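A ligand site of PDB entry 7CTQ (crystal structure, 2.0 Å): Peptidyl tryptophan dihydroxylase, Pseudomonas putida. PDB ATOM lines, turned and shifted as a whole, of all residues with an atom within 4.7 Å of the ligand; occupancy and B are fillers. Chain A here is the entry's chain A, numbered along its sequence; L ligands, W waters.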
ATOM      1  N   GLY A  12     -13.079  22.502  -0.006  1.00  0.00           N
ATOM      2  CA  GLY A  12     -13.629  23.572   0.815  1.00  0.00           C
ATOM      3  C   GLY A  12     -13.928  24.825   0.015  1.00  0.00           C
ATOM      4  O   GLY A  12     -13.094  25.290  -0.789  1.00  0.00           O
ATOM      5  N   ALA A  13     -15.112  25.393   0.212  1.00  0.00           N
ATOM      6  CA  ALA A  13     -15.556  26.529  -0.587  1.00  0.00           C
ATOM      7  C   ALA A  13     -15.874  27.726   0.289  1.00  0.00           C
ATOM      8  O   ALA A  13     -16.898  28.391   0.098  1.00  0.00           O
ATOM      9  CB  ALA A  13     -16.767  26.162  -1.439  1.00  0.00           C
ATOM     10  N   GLY A  14     -15.008  28.010   1.267  1.00  0.00           N
ATOM     11  CA  GLY A  14     -15.082  29.259   1.977  1.00  0.00           C
ATOM     12  C   GLY A  14     -14.387  30.339   1.176  1.00  0.00           C
ATOM     13  O   GLY A  14     -13.985  30.127   0.026  1.00  0.00           O
ATOM     14  N   PRO A  15     -14.218  31.523   1.786  1.00  0.00           N
ATOM     15  CA  PRO A  15     -13.531  32.614   1.071  1.00  0.00           C
ATOM     16  C   PRO A  15     -12.197  32.198   0.470  1.00  0.00           C
ATOM     17  O   PRO A  15     -11.888  32.583  -0.671  1.00  0.00           O
ATOM     18  CB  PRO A  15     -13.352  33.684   2.162  1.00  0.00           C
ATOM     19  CG  PRO A  15     -14.329  33.335   3.213  1.00  0.00           C
ATOM     20  CD  PRO A  15     -14.551  31.867   3.172  1.00  0.00           C
ATOM     21  N   ALA A  16     -11.402  31.419   1.194  1.00  0.00           N
ATOM     22  CA  ALA A  16     -10.048  31.119   0.736  1.00  0.00           C
ATOM     23  C   ALA A  16     -10.045  30.137  -0.429  1.00  0.00           C
ATOM     24  O   ALA A  16      -9.357  30.359  -1.435  1.00  0.00           O
ATOM     25  CB  ALA A  16      -9.221  30.587   1.908  1.00  0.00           C
ATOM     26  N   GLY A  17     -10.767  29.024  -0.297  1.00  0.00           N
ATOM     27  CA  GLY A  17     -10.854  28.081  -1.413  1.00  0.00           C
ATOM     28  C   GLY A  17     -11.463  28.718  -2.645  1.00  0.00           C
ATOM     29  O   GLY A  17     -10.941  28.538  -3.763  1.00  0.00           O
ATOM     30  N   VAL A  34     -14.637  20.922  -4.128  1.00  0.00           N
ATOM     31  CA  VAL A  34     -15.485  20.043  -3.329  1.00  0.00           C
ATOM     32  C   VAL A  34     -15.707  20.700  -1.977  1.00  0.00           C
ATOM     33  O   VAL A  34     -14.744  21.176  -1.370  1.00  0.00           O
ATOM     34  CB  VAL A  34     -14.858  18.653  -3.142  1.00  0.00           C
ATOM     35  CG1 VAL A  34     -15.817  17.727  -2.408  1.00  0.00           C
ATOM     36  CG2 VAL A  34     -14.451  18.068  -4.484  1.00  0.00           C
ATOM     37  N   SER A  35     -16.948  20.717  -1.517  1.00  0.00           N
ATOM     38  CA  SER A  35     -17.234  21.330  -0.219  1.00  0.00           C
ATOM     39  C   SER A  35     -18.629  20.923   0.234  1.00  0.00           C
ATOM     40  O   SER A  35     -19.469  20.502  -0.566  1.00  0.00           O
ATOM     41  CB  SER A  35     -17.121  22.855  -0.276  1.00  0.00           C
ATOM     42  OG  SER A  35     -17.696  23.459   0.872  1.00  0.00           O
ATOM     43  N   GLU A  36     -18.858  21.086   1.532  1.00  0.00           N
ATOM     44  CA  GLU A  36     -20.125  20.726   2.144  1.00  0.00           C
ATOM     45  C   GLU A  36     -21.072  21.925   2.127  1.00  0.00           C
ATOM     46  O   GLU A  36     -20.646  23.074   2.281  1.00  0.00           O
ATOM     47  CB  GLU A  36     -19.905  20.242   3.583  1.00  0.00           C
ATOM     48  CG  GLU A  36     -21.189  20.026   4.380  1.00  0.00           C
ATOM     49  CD  GLU A  36     -21.062  18.907   5.384  1.00  0.00           C
ATOM     50  OE1 GLU A  36     -20.238  17.998   5.165  1.00  0.00           O
ATOM     51  OE2 GLU A  36     -21.791  18.937   6.401  1.00  0.00           O
ATOM     52  N   ARG A  38     -23.566  23.389   3.985  1.00  0.00           N
ATOM     53  CA  ARG A  38     -23.790  24.369   5.034  1.00  0.00           C
ATOM     54  C   ARG A  38     -23.198  23.892   6.351  1.00  0.00           C
ATOM     55  O   ARG A  38     -22.633  22.797   6.453  1.00  0.00           O
ATOM     56  CB  ARG A  38     -25.289  24.643   5.217  1.00  0.00           C
ATOM     57  CG  ARG A  38     -25.988  25.143   3.957  1.00  0.00           C
ATOM     58  CD  ARG A  38     -27.501  25.236   4.108  1.00  0.00           C
ATOM     59  NE  ARG A  38     -27.932  25.565   5.466  1.00  0.00           N
ATOM     60  CZ  ARG A  38     -27.654  26.701   6.097  1.00  0.00           C
ATOM     61  NH1 ARG A  38     -26.945  27.644   5.494  1.00  0.00           N
ATOM     62  NH2 ARG A  38     -28.096  26.908   7.332  1.00  0.00           N
ATOM     63  N   GLU A  44     -21.003  37.138  11.184  1.00  0.00           N
ATOM     64  CA  GLU A  44     -19.734  37.743  11.524  1.00  0.00           C
ATOM     65  C   GLU A  44     -19.801  39.228  11.237  1.00  0.00           C
ATOM     66  O   GLU A  44     -20.617  39.696  10.449  1.00  0.00           O
ATOM     67  CB  GLU A  44     -18.603  37.087  10.720  1.00  0.00           C
ATOM     68  CG  GLU A  44     -18.242  35.700  11.207  1.00  0.00           C
ATOM     69  CD  GLU A  44     -17.486  34.883  10.180  1.00  0.00           C
ATOM     70  OE1 GLU A  44     -17.055  33.756  10.531  1.00  0.00           O
ATOM     71  OE2 GLU A  44     -17.337  35.347   9.028  1.00  0.00           O
ATOM     72  N   GLY A  45     -18.930  39.985  11.918  1.00  0.00           N
ATOM     73  CA  GLY A  45     -18.776  41.394  11.632  1.00  0.00           C
ATOM     74  C   GLY A  45     -17.748  41.587  10.528  1.00  0.00           C
ATOM     75  O   GLY A  45     -16.658  41.019  10.576  1.00  0.00           O
ATOM     76  N   VAL A  46     -18.119  42.383   9.521  1.00  0.00           N
ATOM     77  CA  VAL A  46     -17.232  42.657   8.399  1.00  0.00           C
ATOM     78  C   VAL A  46     -17.075  44.167   8.263  1.00  0.00           C
ATOM     79  O   VAL A  46     -18.002  44.935   8.529  1.00  0.00           O
ATOM     80  CB  VAL A  46     -17.747  42.038   7.077  1.00  0.00           C
ATOM     81  CG1 VAL A  46     -17.587  40.519   7.114  1.00  0.00           C
ATOM     82  CG2 VAL A  46     -19.192  42.439   6.805  1.00  0.00           C
ATOM     83  N   ARG A  91     -23.047  33.907   7.275  1.00  0.00           N
ATOM     84  CA  ARG A  91     -22.245  32.879   6.623  1.00  0.00           C
ATOM     85  C   ARG A  91     -23.101  31.811   5.963  1.00  0.00           C
ATOM     86  O   ARG A  91     -22.642  31.161   5.027  1.00  0.00           O
ATOM     87  CB  ARG A  91     -21.302  32.241   7.642  1.00  0.00           C
ATOM     88  CG  ARG A  91     -20.246  33.203   8.168  1.00  0.00           C
ATOM     89  CD  ARG A  91     -19.439  33.768   7.022  1.00  0.00           C
ATOM     90  NE  ARG A  91     -18.834  32.730   6.206  1.00  0.00           N
ATOM     91  CZ  ARG A  91     -17.586  32.280   6.363  1.00  0.00           C
ATOM     92  NH1 ARG A  91     -16.820  32.811   7.314  1.00  0.00           N
ATOM     93  NH2 ARG A  91     -17.107  31.321   5.592  1.00  0.00           N
ATOM     94  N   GLY A 112     -20.447  17.791  -1.231  1.00  0.00           N
ATOM     95  CA  GLY A 112     -20.156  16.568  -0.500  1.00  0.00           C
ATOM     96  C   GLY A 112     -19.095  16.738   0.569  1.00  0.00           C
ATOM     97  O   GLY A 112     -18.163  17.532   0.432  1.00  0.00           O
ATOM     98  N   ARG A 113     -19.234  15.993   1.657  1.00  0.00           N
ATOM     99  CA  ARG A 113     -18.210  15.966   2.689  1.00  0.00           C
ATOM    100  C   ARG A 113     -17.086  15.026   2.273  1.00  0.00           C
ATOM    101  O   ARG A 113     -17.330  13.908   1.804  1.00  0.00           O
ATOM    102  CB  ARG A 113     -18.800  15.521   4.034  1.00  0.00           C
ATOM    103  CG  ARG A 113     -17.728  15.206   5.065  1.00  0.00           C
ATOM    104  CD  ARG A 113     -18.171  15.551   6.473  1.00  0.00           C
ATOM    105  NE  ARG A 113     -19.010  14.503   7.038  1.00  0.00           N
ATOM    106  CZ  ARG A 113     -19.551  14.559   8.251  1.00  0.00           C
ATOM    107  NH1 ARG A 113     -20.310  13.553   8.673  1.00  0.00           N
ATOM    108  NH2 ARG A 113     -19.350  15.613   9.027  1.00  0.00           N
ATOM    109  N   VAL A 114     -15.847  15.485   2.446  1.00  0.00           N
ATOM    110  CA  VAL A 114     -14.683  14.654   2.142  1.00  0.00           C
ATOM    111  C   VAL A 114     -14.474  13.676   3.284  1.00  0.00           C
ATOM    112  O   VAL A 114     -14.419  14.066   4.462  1.00  0.00           O
ATOM    113  CB  VAL A 114     -13.434  15.509   1.917  1.00  0.00           C
ATOM    114  CG1 VAL A 114     -12.267  14.636   1.485  1.00  0.00           C
ATOM    115  CG2 VAL A 114     -13.708  16.587   0.869  1.00  0.00           C
ATOM    116  N   ALA A 141      -8.401  23.740   1.689  1.00  0.00           N
ATOM    117  CA  ALA A 141      -9.031  24.997   2.028  1.00  0.00           C
ATOM    118  C   ALA A 141     -10.238  24.764   2.903  1.00  0.00           C
ATOM    119  O   ALA A 141     -11.233  25.493   2.817  1.00  0.00           O
ATOM    120  CB  ALA A 141      -9.421  25.770   0.763  1.00  0.00           C
ATOM    121  N   ARG A 142     -10.183  23.759   3.773  1.00  0.00           N
ATOM    122  CA  ARG A 142     -11.319  23.466   4.631  1.00  0.00           C
ATOM    123  C   ARG A 142     -11.290  24.224   5.948  1.00  0.00           C
ATOM    124  O   ARG A 142     -11.930  23.797   6.914  1.00  0.00           O
ATOM    125  CB  ARG A 142     -11.432  21.967   4.901  1.00  0.00           C
ATOM    126  CG  ARG A 142     -11.670  21.139   3.645  1.00  0.00           C
ATOM    127  CD  ARG A 142     -11.806  19.685   3.997  1.00  0.00           C
ATOM    128  NE  ARG A 142     -10.607  18.946   3.632  1.00  0.00           N
ATOM    129  CZ  ARG A 142     -10.107  17.952   4.350  1.00  0.00           C
ATOM    130  NH1 ARG A 142     -10.721  17.571   5.462  1.00  0.00           N
ATOM    131  NH2 ARG A 142      -8.997  17.338   3.942  1.00  0.00           N
ATOM    132  N   GLY A 143     -10.554  25.335   6.010  1.00  0.00           N
ATOM    133  CA  GLY A 143     -10.607  26.172   7.192  1.00  0.00           C
ATOM    134  C   GLY A 143     -10.032  25.475   8.413  1.00  0.00           C
ATOM    135  O   GLY A 143      -9.155  24.613   8.329  1.00  0.00           O
ATOM    136  N   ARG A 144     -10.553  25.871   9.588  1.00  0.00           N
ATOM    137  CA  ARG A 144     -10.160  25.203  10.820  1.00  0.00           C
ATOM    138  C   ARG A 144     -10.579  23.732  10.852  1.00  0.00           C
ATOM    139  O   ARG A 144     -10.027  22.966  11.643  1.00  0.00           O
ATOM    140  CB  ARG A 144     -10.729  25.967  12.028  1.00  0.00           C
ATOM    141  CG  ARG A 144     -10.117  27.352  12.216  1.00  0.00           C
ATOM    142  CD  ARG A 144     -10.591  28.008  13.510  1.00  0.00           C
ATOM    143  NE  ARG A 144      -9.991  29.313  13.817  1.00  0.00           N
ATOM    144  CZ  ARG A 144      -9.022  29.501  14.715  1.00  0.00           C
ATOM    145  NH1 ARG A 144      -8.546  30.730  14.949  1.00  0.00           N
ATOM    146  NH2 ARG A 144      -8.513  28.476  15.370  1.00  0.00           N
ATOM    147  N   GLN A 145     -11.493  23.316  10.005  1.00  0.00           N
ATOM    148  CA  GLN A 145     -11.847  21.893   9.937  1.00  0.00           C
ATOM    149  C   GLN A 145     -10.812  21.090   9.170  1.00  0.00           C
ATOM    150  O   GLN A 145     -11.061  19.906   8.916  1.00  0.00           O
ATOM    151  CB  GLN A 145     -13.269  21.702   9.332  1.00  0.00           C
ATOM    152  CG  GLN A 145     -14.304  22.642   9.881  1.00  0.00           C
ATOM    153  CD  GLN A 145     -15.666  22.514   9.192  1.00  0.00           C
ATOM    154  OE1 GLN A 145     -16.149  21.411   8.934  1.00  0.00           O
ATOM    155  NE2 GLN A 145     -16.253  23.644   8.858  1.00  0.00           N
ATOM    156  N   SER A 160     -14.183  30.154  21.729  1.00  0.00           N
ATOM    157  CA  SER A 160     -15.300  31.052  21.525  1.00  0.00           C
ATOM    158  C   SER A 160     -16.574  30.228  21.720  1.00  0.00           C
ATOM    159  O   SER A 160     -16.762  29.210  21.058  1.00  0.00           O
ATOM    160  CB  SER A 160     -15.247  31.695  20.136  1.00  0.00           C
ATOM    161  OG  SER A 160     -14.129  32.584  20.045  1.00  0.00           O
ATOM    162  N   GLN A 197     -21.455  35.438  21.161  1.00  0.00           N
ATOM    163  CA  GLN A 197     -20.227  34.662  21.125  1.00  0.00           C
ATOM    164  C   GLN A 197     -19.232  35.295  22.065  1.00  0.00           C
ATOM    165  O   GLN A 197     -18.898  36.484  21.923  1.00  0.00           O
ATOM    166  CB  GLN A 197     -19.689  34.586  19.692  1.00  0.00           C
ATOM    167  CG  GLN A 197     -18.182  34.558  19.561  1.00  0.00           C
ATOM    168  CD  GLN A 197     -17.750  35.090  18.211  1.00  0.00           C
ATOM    169  OE1 GLN A 197     -18.110  34.534  17.165  1.00  0.00           O
ATOM    170  NE2 GLN A 197     -16.986  36.186  18.231  1.00  0.00           N
ATOM    171  N   ARG A 242     -16.219  26.787  19.814  1.00  0.00           N
ATOM    172  CA  ARG A 242     -15.278  26.873  18.693  1.00  0.00           C
ATOM    173  C   ARG A 242     -13.884  27.131  19.242  1.00  0.00           C
ATOM    174  O   ARG A 242     -13.695  28.057  20.050  1.00  0.00           O
ATOM    175  CB  ARG A 242     -15.641  28.006  17.723  1.00  0.00           C
ATOM    176  CG  ARG A 242     -16.979  27.850  17.011  1.00  0.00           C
ATOM    177  CD  ARG A 242     -16.976  28.481  15.606  1.00  0.00           C
ATOM    178  NE  ARG A 242     -17.930  29.589  15.508  1.00  0.00           N
ATOM    179  CZ  ARG A 242     -17.768  30.688  14.756  1.00  0.00           C
ATOM    180  NH1 ARG A 242     -16.702  30.824  13.970  1.00  0.00           N
ATOM    181  NH2 ARG A 242     -18.693  31.627  14.761  1.00  0.00           N
ATOM    182  N   SER A 243     -12.917  26.341  18.808  1.00  0.00           N
ATOM    183  CA  SER A 243     -11.531  26.715  19.036  1.00  0.00           C
ATOM    184  C   SER A 243     -11.215  27.972  18.230  1.00  0.00           C
ATOM    185  O   SER A 243     -11.437  28.000  17.015  1.00  0.00           O
ATOM    186  CB  SER A 243     -10.576  25.580  18.660  1.00  0.00           C
ATOM    187  OG  SER A 243      -9.218  25.998  18.827  1.00  0.00           O
ATOM    188  N   SER A 244     -10.761  29.018  18.910  1.00  0.00           N
ATOM    189  CA  SER A 244     -10.394  30.272  18.252  1.00  0.00           C
ATOM    190  C   SER A 244      -8.937  30.632  18.521  1.00  0.00           C
ATOM    191  O   SER A 244      -8.558  31.807  18.432  1.00  0.00           O
ATOM    192  CB  SER A 244     -11.322  31.399  18.694  1.00  0.00           C
ATOM    193  OG  SER A 244     -11.278  31.532  20.098  1.00  0.00           O
ATOM    194  N   VAL A 260      -4.434  26.880   2.167  1.00  0.00           N
ATOM    195  CA  VAL A 260      -4.784  28.292   2.102  1.00  0.00           C
ATOM    196  C   VAL A 260      -5.805  28.603   3.183  1.00  0.00           C
ATOM    197  O   VAL A 260      -6.467  27.709   3.723  1.00  0.00           O
ATOM    198  CB  VAL A 260      -5.335  28.705   0.720  1.00  0.00           C
ATOM    199  CG1 VAL A 260      -4.258  28.556  -0.336  1.00  0.00           C
ATOM    200  CG2 VAL A 260      -6.582  27.893   0.351  1.00  0.00           C
ATOM    201  N   GLY A 261      -5.912  29.884   3.505  1.00  0.00           N
ATOM    202  CA  GLY A 261      -6.911  30.296   4.468  1.00  0.00           C
ATOM    203  C   GLY A 261      -6.596  29.846   5.881  1.00  0.00           C
ATOM    204  O   GLY A 261      -5.436  29.708   6.284  1.00  0.00           O
ATOM    205  N   ASP A 262      -7.675  29.623   6.648  1.00  0.00           N
ATOM    206  CA  ASP A 262      -7.564  29.170   8.038  1.00  0.00           C
ATOM    207  C   ASP A 262      -6.776  27.858   8.152  1.00  0.00           C
ATOM    208  O   ASP A 262      -6.133  27.603   9.176  1.00  0.00           O
ATOM    209  CB  ASP A 262      -8.950  28.979   8.645  1.00  0.00           C
ATOM    210  CG  ASP A 262      -9.526  30.248   9.245  1.00  0.00           C
ATOM    211  OD1 ASP A 262      -8.912  31.328   9.060  1.00  0.00           O
ATOM    212  OD2 ASP A 262     -10.596  30.168   9.896  1.00  0.00           O
ATOM    213  N   ALA A 263      -6.842  27.007   7.127  1.00  0.00           N
ATOM    214  CA  ALA A 263      -6.020  25.811   7.102  1.00  0.00           C
ATOM    215  C   ALA A 263      -4.538  26.137   7.111  1.00  0.00           C
ATOM    216  O   ALA A 263      -3.725  25.290   7.504  1.00  0.00           O
ATOM    217  CB  ALA A 263      -6.340  24.965   5.882  1.00  0.00           C
ATOM    218  N   PRO A 269     -10.444  36.029  16.503  1.00  0.00           N
ATOM    219  CA  PRO A 269     -11.343  36.883  15.723  1.00  0.00           C
ATOM    220  C   PRO A 269     -11.530  38.297  16.235  1.00  0.00           C
ATOM    221  O   PRO A 269     -12.423  38.990  15.735  1.00  0.00           O
ATOM    222  CB  PRO A 269     -12.673  36.126  15.790  1.00  0.00           C
ATOM    223  CG  PRO A 269     -12.627  35.459  17.125  1.00  0.00           C
ATOM    224  CD  PRO A 269     -11.208  34.998  17.251  1.00  0.00           C
ATOM    225  N   GLY A 272     -12.209  41.513  13.848  1.00  0.00           N
ATOM    226  CA  GLY A 272     -13.337  41.661  12.947  1.00  0.00           C
ATOM    227  C   GLY A 272     -12.927  41.609  11.496  1.00  0.00           C
ATOM    228  O   GLY A 272     -13.646  42.146  10.640  1.00  0.00           O
ATOM    229  N   ASN A 273     -11.791  40.976  11.202  1.00  0.00           N
ATOM    230  CA  ASN A 273     -11.185  41.046   9.875  1.00  0.00           C
ATOM    231  C   ASN A 273     -10.710  39.691   9.385  1.00  0.00           C
ATOM    232  O   ASN A 273      -9.881  39.638   8.476  1.00  0.00           O
ATOM    233  CB  ASN A 273     -10.008  42.023   9.883  1.00  0.00           C
ATOM    234  CG  ASN A 273     -10.376  43.387   9.377  1.00  0.00           C
ATOM    235  OD1 ASN A 273     -10.111  43.726   8.227  1.00  0.00           O
ATOM    236  ND2 ASN A 273     -11.007  44.191  10.232  1.00  0.00           N
ATOM    237  N   GLY A 274     -11.232  38.596   9.948  1.00  0.00           N
ATOM    238  CA  GLY A 274     -10.699  37.283   9.630  1.00  0.00           C
ATOM    239  C   GLY A 274     -10.839  36.906   8.172  1.00  0.00           C
ATOM    240  O   GLY A 274      -9.920  36.331   7.570  1.00  0.00           O
ATOM    241  N   ILE A 275     -11.986  37.232   7.562  1.00  0.00           N
ATOM    242  CA  ILE A 275     -12.199  36.867   6.164  1.00  0.00           C
ATOM    243  C   ILE A 275     -11.161  37.542   5.274  1.00  0.00           C
ATOM    244  O   ILE A 275     -10.623  36.926   4.349  1.00  0.00           O
ATOM    245  CB  ILE A 275     -13.638  37.217   5.741  1.00  0.00           C
ATOM    246  CG1 ILE A 275     -14.633  36.217   6.351  1.00  0.00           C
ATOM    247  CG2 ILE A 275     -13.757  37.180   4.244  1.00  0.00           C
ATOM    248  CD1 ILE A 275     -16.082  36.691   6.366  1.00  0.00           C
ATOM    249  N   SER A 278      -7.873  35.757   5.740  1.00  0.00           N
ATOM    250  CA  SER A 278      -7.878  34.487   5.018  1.00  0.00           C
ATOM    251  C   SER A 278      -7.708  34.699   3.519  1.00  0.00           C
ATOM    252  O   SER A 278      -7.024  33.918   2.848  1.00  0.00           O
ATOM    253  CB  SER A 278      -9.155  33.711   5.317  1.00  0.00           C
ATOM    254  OG  SER A 278      -9.616  34.035   6.627  1.00  0.00           O
HETATM  255  P1  LIG L   1     -13.994  28.521   5.927  1.00  0.00           P
HETATM  256  O1  LIG L   1     -14.663  29.808   5.705  1.00  0.00           O
HETATM  257  O2  LIG L   1     -14.236  27.935   7.312  1.00  0.00           O
HETATM  258  O3  LIG L   1     -14.343  27.555   4.752  1.00  0.00           O
HETATM  259  C1  LIG L   1     -14.176  26.125   4.870  1.00  0.00           C
HETATM  260  C2  LIG L   1     -15.239  25.505   4.003  1.00  0.00           C
HETATM  261  O4  LIG L   1     -14.981  24.084   3.899  1.00  0.00           O
HETATM  262  C3  LIG L   1     -16.674  25.646   4.509  1.00  0.00           C
HETATM  263  O5  LIG L   1     -17.559  25.865   3.418  1.00  0.00           O
HETATM  264  C4  LIG L   1     -16.927  24.303   5.220  1.00  0.00           C
HETATM  265  O6  LIG L   1     -18.293  23.907   5.193  1.00  0.00           O
HETATM  266  C5  LIG L   1     -16.107  23.356   4.332  1.00  0.00           C
HETATM  267  N1  LIG L   1     -15.675  22.109   4.931  1.00  0.00           N
HETATM  268  C6  LIG L   1     -15.232  21.866   6.204  1.00  0.00           C
HETATM  269  N2  LIG L   1     -14.889  20.627   6.433  1.00  0.00           N
HETATM  270  C7  LIG L   1     -15.167  19.998   5.237  1.00  0.00           C
HETATM  271  C8  LIG L   1     -15.041  18.656   4.821  1.00  0.00           C
HETATM  272  N3  LIG L   1     -14.602  17.668   5.601  1.00  0.00           N
HETATM  273  N4  LIG L   1     -15.392  18.351   3.542  1.00  0.00           N
HETATM  274  C9  LIG L   1     -15.836  19.324   2.749  1.00  0.00           C
HETATM  275  N5  LIG L   1     -15.988  20.629   3.042  1.00  0.00           N
HETATM  276  C10 LIG L   1     -15.634  20.897   4.300  1.00  0.00           C
HETATM  277  N6  LIG L   1     -13.967  36.680  10.246  1.00  0.00           N
HETATM  278  C11 LIG L   1     -14.486  37.910   9.959  1.00  0.00           C
HETATM  279  O7  LIG L   1     -14.215  38.496   8.908  1.00  0.00           O
HETATM  280  N7  LIG L   1     -15.365  38.511  10.842  1.00  0.00           N
HETATM  281  C12 LIG L   1     -15.782  37.987  12.047  1.00  0.00           C
HETATM  282  O8  LIG L   1     -16.577  38.620  12.746  1.00  0.00           O
HETATM  283  C13 LIG L   1     -15.231  36.682  12.349  1.00  0.00           C
HETATM  284  N8  LIG L   1     -15.571  36.123  13.473  1.00  0.00           N
HETATM  285  C14 LIG L   1     -15.037  34.881  13.769  1.00  0.00           C
HETATM  286  C15 LIG L   1     -15.394  34.261  14.974  1.00  0.00           C
HETATM  287  C16 LIG L   1     -14.872  33.020  15.321  1.00  0.00           C
HETATM  288  C17 LIG L   1     -15.274  32.375  16.623  1.00  0.00           C
HETATM  289  C18 LIG L   1     -13.974  32.379  14.450  1.00  0.00           C
HETATM  290  C19 LIG L   1     -13.403  31.021  14.795  1.00  0.00           C
HETATM  291  C20 LIG L   1     -13.625  32.984  13.250  1.00  0.00           C
HETATM  292  C21 LIG L   1     -14.147  34.224  12.903  1.00  0.00           C
HETATM  293  N9  LIG L   1     -13.812  34.863  11.698  1.00  0.00           N
HETATM  294  C22 LIG L   1     -14.328  36.107  11.394  1.00  0.00           C
HETATM  295  C23 LIG L   1     -12.848  34.252  10.782  1.00  0.00           C
HETATM  296  C24 LIG L   1     -13.461  33.638   9.538  1.00  0.00           C
HETATM  297  O9  LIG L   1     -14.546  32.758   9.868  1.00  0.00           O
HETATM  298  C25 LIG L   1     -12.381  32.862   8.804  1.00  0.00           C
HETATM  299  O10 LIG L   1     -11.225  33.697   8.718  1.00  0.00           O
HETATM  300  C26 LIG L   1     -12.728  32.407   7.384  1.00  0.00           C
HETATM  301  O11 LIG L   1     -14.063  31.904   7.315  1.00  0.00           O
HETATM  302  C27 LIG L   1     -11.748  31.367   6.898  1.00  0.00           C
HETATM  303  O12 LIG L   1     -11.997  31.113   5.504  1.00  0.00           O
HETATM  304  P2  LIG L   1     -11.658  29.732   4.866  1.00  0.00           P
HETATM  305  O13 LIG L   1     -10.151  29.516   5.050  1.00  0.00           O
HETATM  306  O14 LIG L   1     -12.185  29.656   3.478  1.00  0.00           O
HETATM  307  O15 LIG L   1     -12.419  28.705   5.803  1.00  0.00           O
HETATM  308  O   HOH W   1     -10.853  31.539  12.120  1.00  0.00           O
HETATM  309  O   HOH W   2     -12.245  27.955   9.270  1.00  0.00           O
HETATM  310  O   HOH W   3      -8.828  27.194   4.681  1.00  0.00           O
HETATM  311  O   HOH W   4     -12.118  27.673   1.478  1.00  0.00           O
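NH2 of Arg 91 lies within salt-bridge range of O1 of the ligand, at 2.9 Å.
The backbone NH (N) of Val 114 lies within hydrogen-bond range of a nitrogen (N4) of the ligand.
An oxygen (O7) of the ligand lies within hydrogen-bond range of the backbone NH (N) of Gly 274, at 3.2 Å.
The side-chain carboxylate (OE1) of Glu 44 sits at hydrogen-bond distance from an oxygen (O9) of the ligand (2.8 Å).
The backbone NH of Ile 275 is in hydrogen-bond range of an oxygen (O7) of the ligand.
O of Gly 274 sits at hydrogen-bond distance from O10 of the ligand (3.2 Å).
N of Ala 16 lies within hydrogen-bond range of O14 of the ligand (3.0 Å).
An oxygen (O10) of the ligand sits at hydrogen-bond distance from the side-chain carboxylate (OD1) of Asp 262 (3.3 Å).
O13 of the ligand is in hydrogen-bond range of N of Asp 262, at 2.9 Å.
OG of Ser 278 sits at hydrogen-bond distance from O10 of the ligand (2.7 Å).
A nitrogen (N5) of the ligand is in hydrogen-bond range of the backbone NH (N) of Glu 36, 3.3 Å away.
OE1 of Gln 145 lies close to N2 of the ligand.
N of Gly 45 is in hydrogen-bond range of O8 of the ligand (2.8 Å).
A nitrogen (N7) of the ligand is in hydrogen-bond range of the backbone carbonyl oxygen (O) of Gly 45, 2.8 Å away.
The side-chain hydroxyl (OG) of Ser 278 is in hydrogen-bond range of the backbone carbonyl oxygen (O) of Gly 274.
The side-chain carboxylate (OE2) of Glu 44 is in salt-bridge range of the guanidinium group (NH1) of Arg 91.
The backbone carbonyl oxygen of Ser 35 is in hydrogen-bond range of the backbone NH of Gly 112 (3.0 Å).
The side-chain hydroxyl (OG) of Ser 35 lies close to the backbone NH (N) of Ala 13 (3.3 Å).
OG of Ser 244 lies within hydrogen-bond range of OG of Ser 160, at 3.0 Å.
The guanidinium group of Arg 144 lies within hydrogen-bond range of the backbone carbonyl oxygen of Ser 243 (3.4 Å).
The backbone NH (N) of Ser 160 is in hydrogen-bond range of the backbone carbonyl oxygen (O) of Arg 242, at 2.7 Å.
The backbone carbonyl oxygen (O) of Val 34 sits at hydrogen-bond distance from the backbone NH (N) of Gly 12 (2.5 Å).
N of Pro 15 lies close to O14 of the ligand (3.2 Å).
Merely in contact with the ligand: Gly 12, Ala 13, Gly 14, Ser 35, Gly 112, Arg 113, Ala 141, Arg 142, Gly 143, Arg 144, Ser 160, Gln 197, Arg 242, Gly 261, Pro 269, Gly 272 and Asn 273.
Hydrophobic or aromatic side chains within 4 Å of the ligand: Pro 15, Ala 16, Val 114, Pro 269 and Ile 275.
The nearest printed residue that does not touch the ligand is Gly 17 (4.1 Å).
Water W2 lies within hydrogen-bond range of the backbone NH of Arg 144 (2.7 Å), an oxygen (O2) of the ligand (2.8 Å) and the side-chain carboxylate of Asp 262 (2.8 Å).
Water W4 lies within hydrogen-bond range of N of Gly 17 (2.6 Å), O of Ala 141 (2.7 Å), O14 of the ligand (2.8 Å), N of Gly 14 (2.9 Å) and O of Gly 12 (3.4 Å).
Water W1 lies within hydrogen-bond range of OD2 of Asp 262 and NE of Arg 144.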
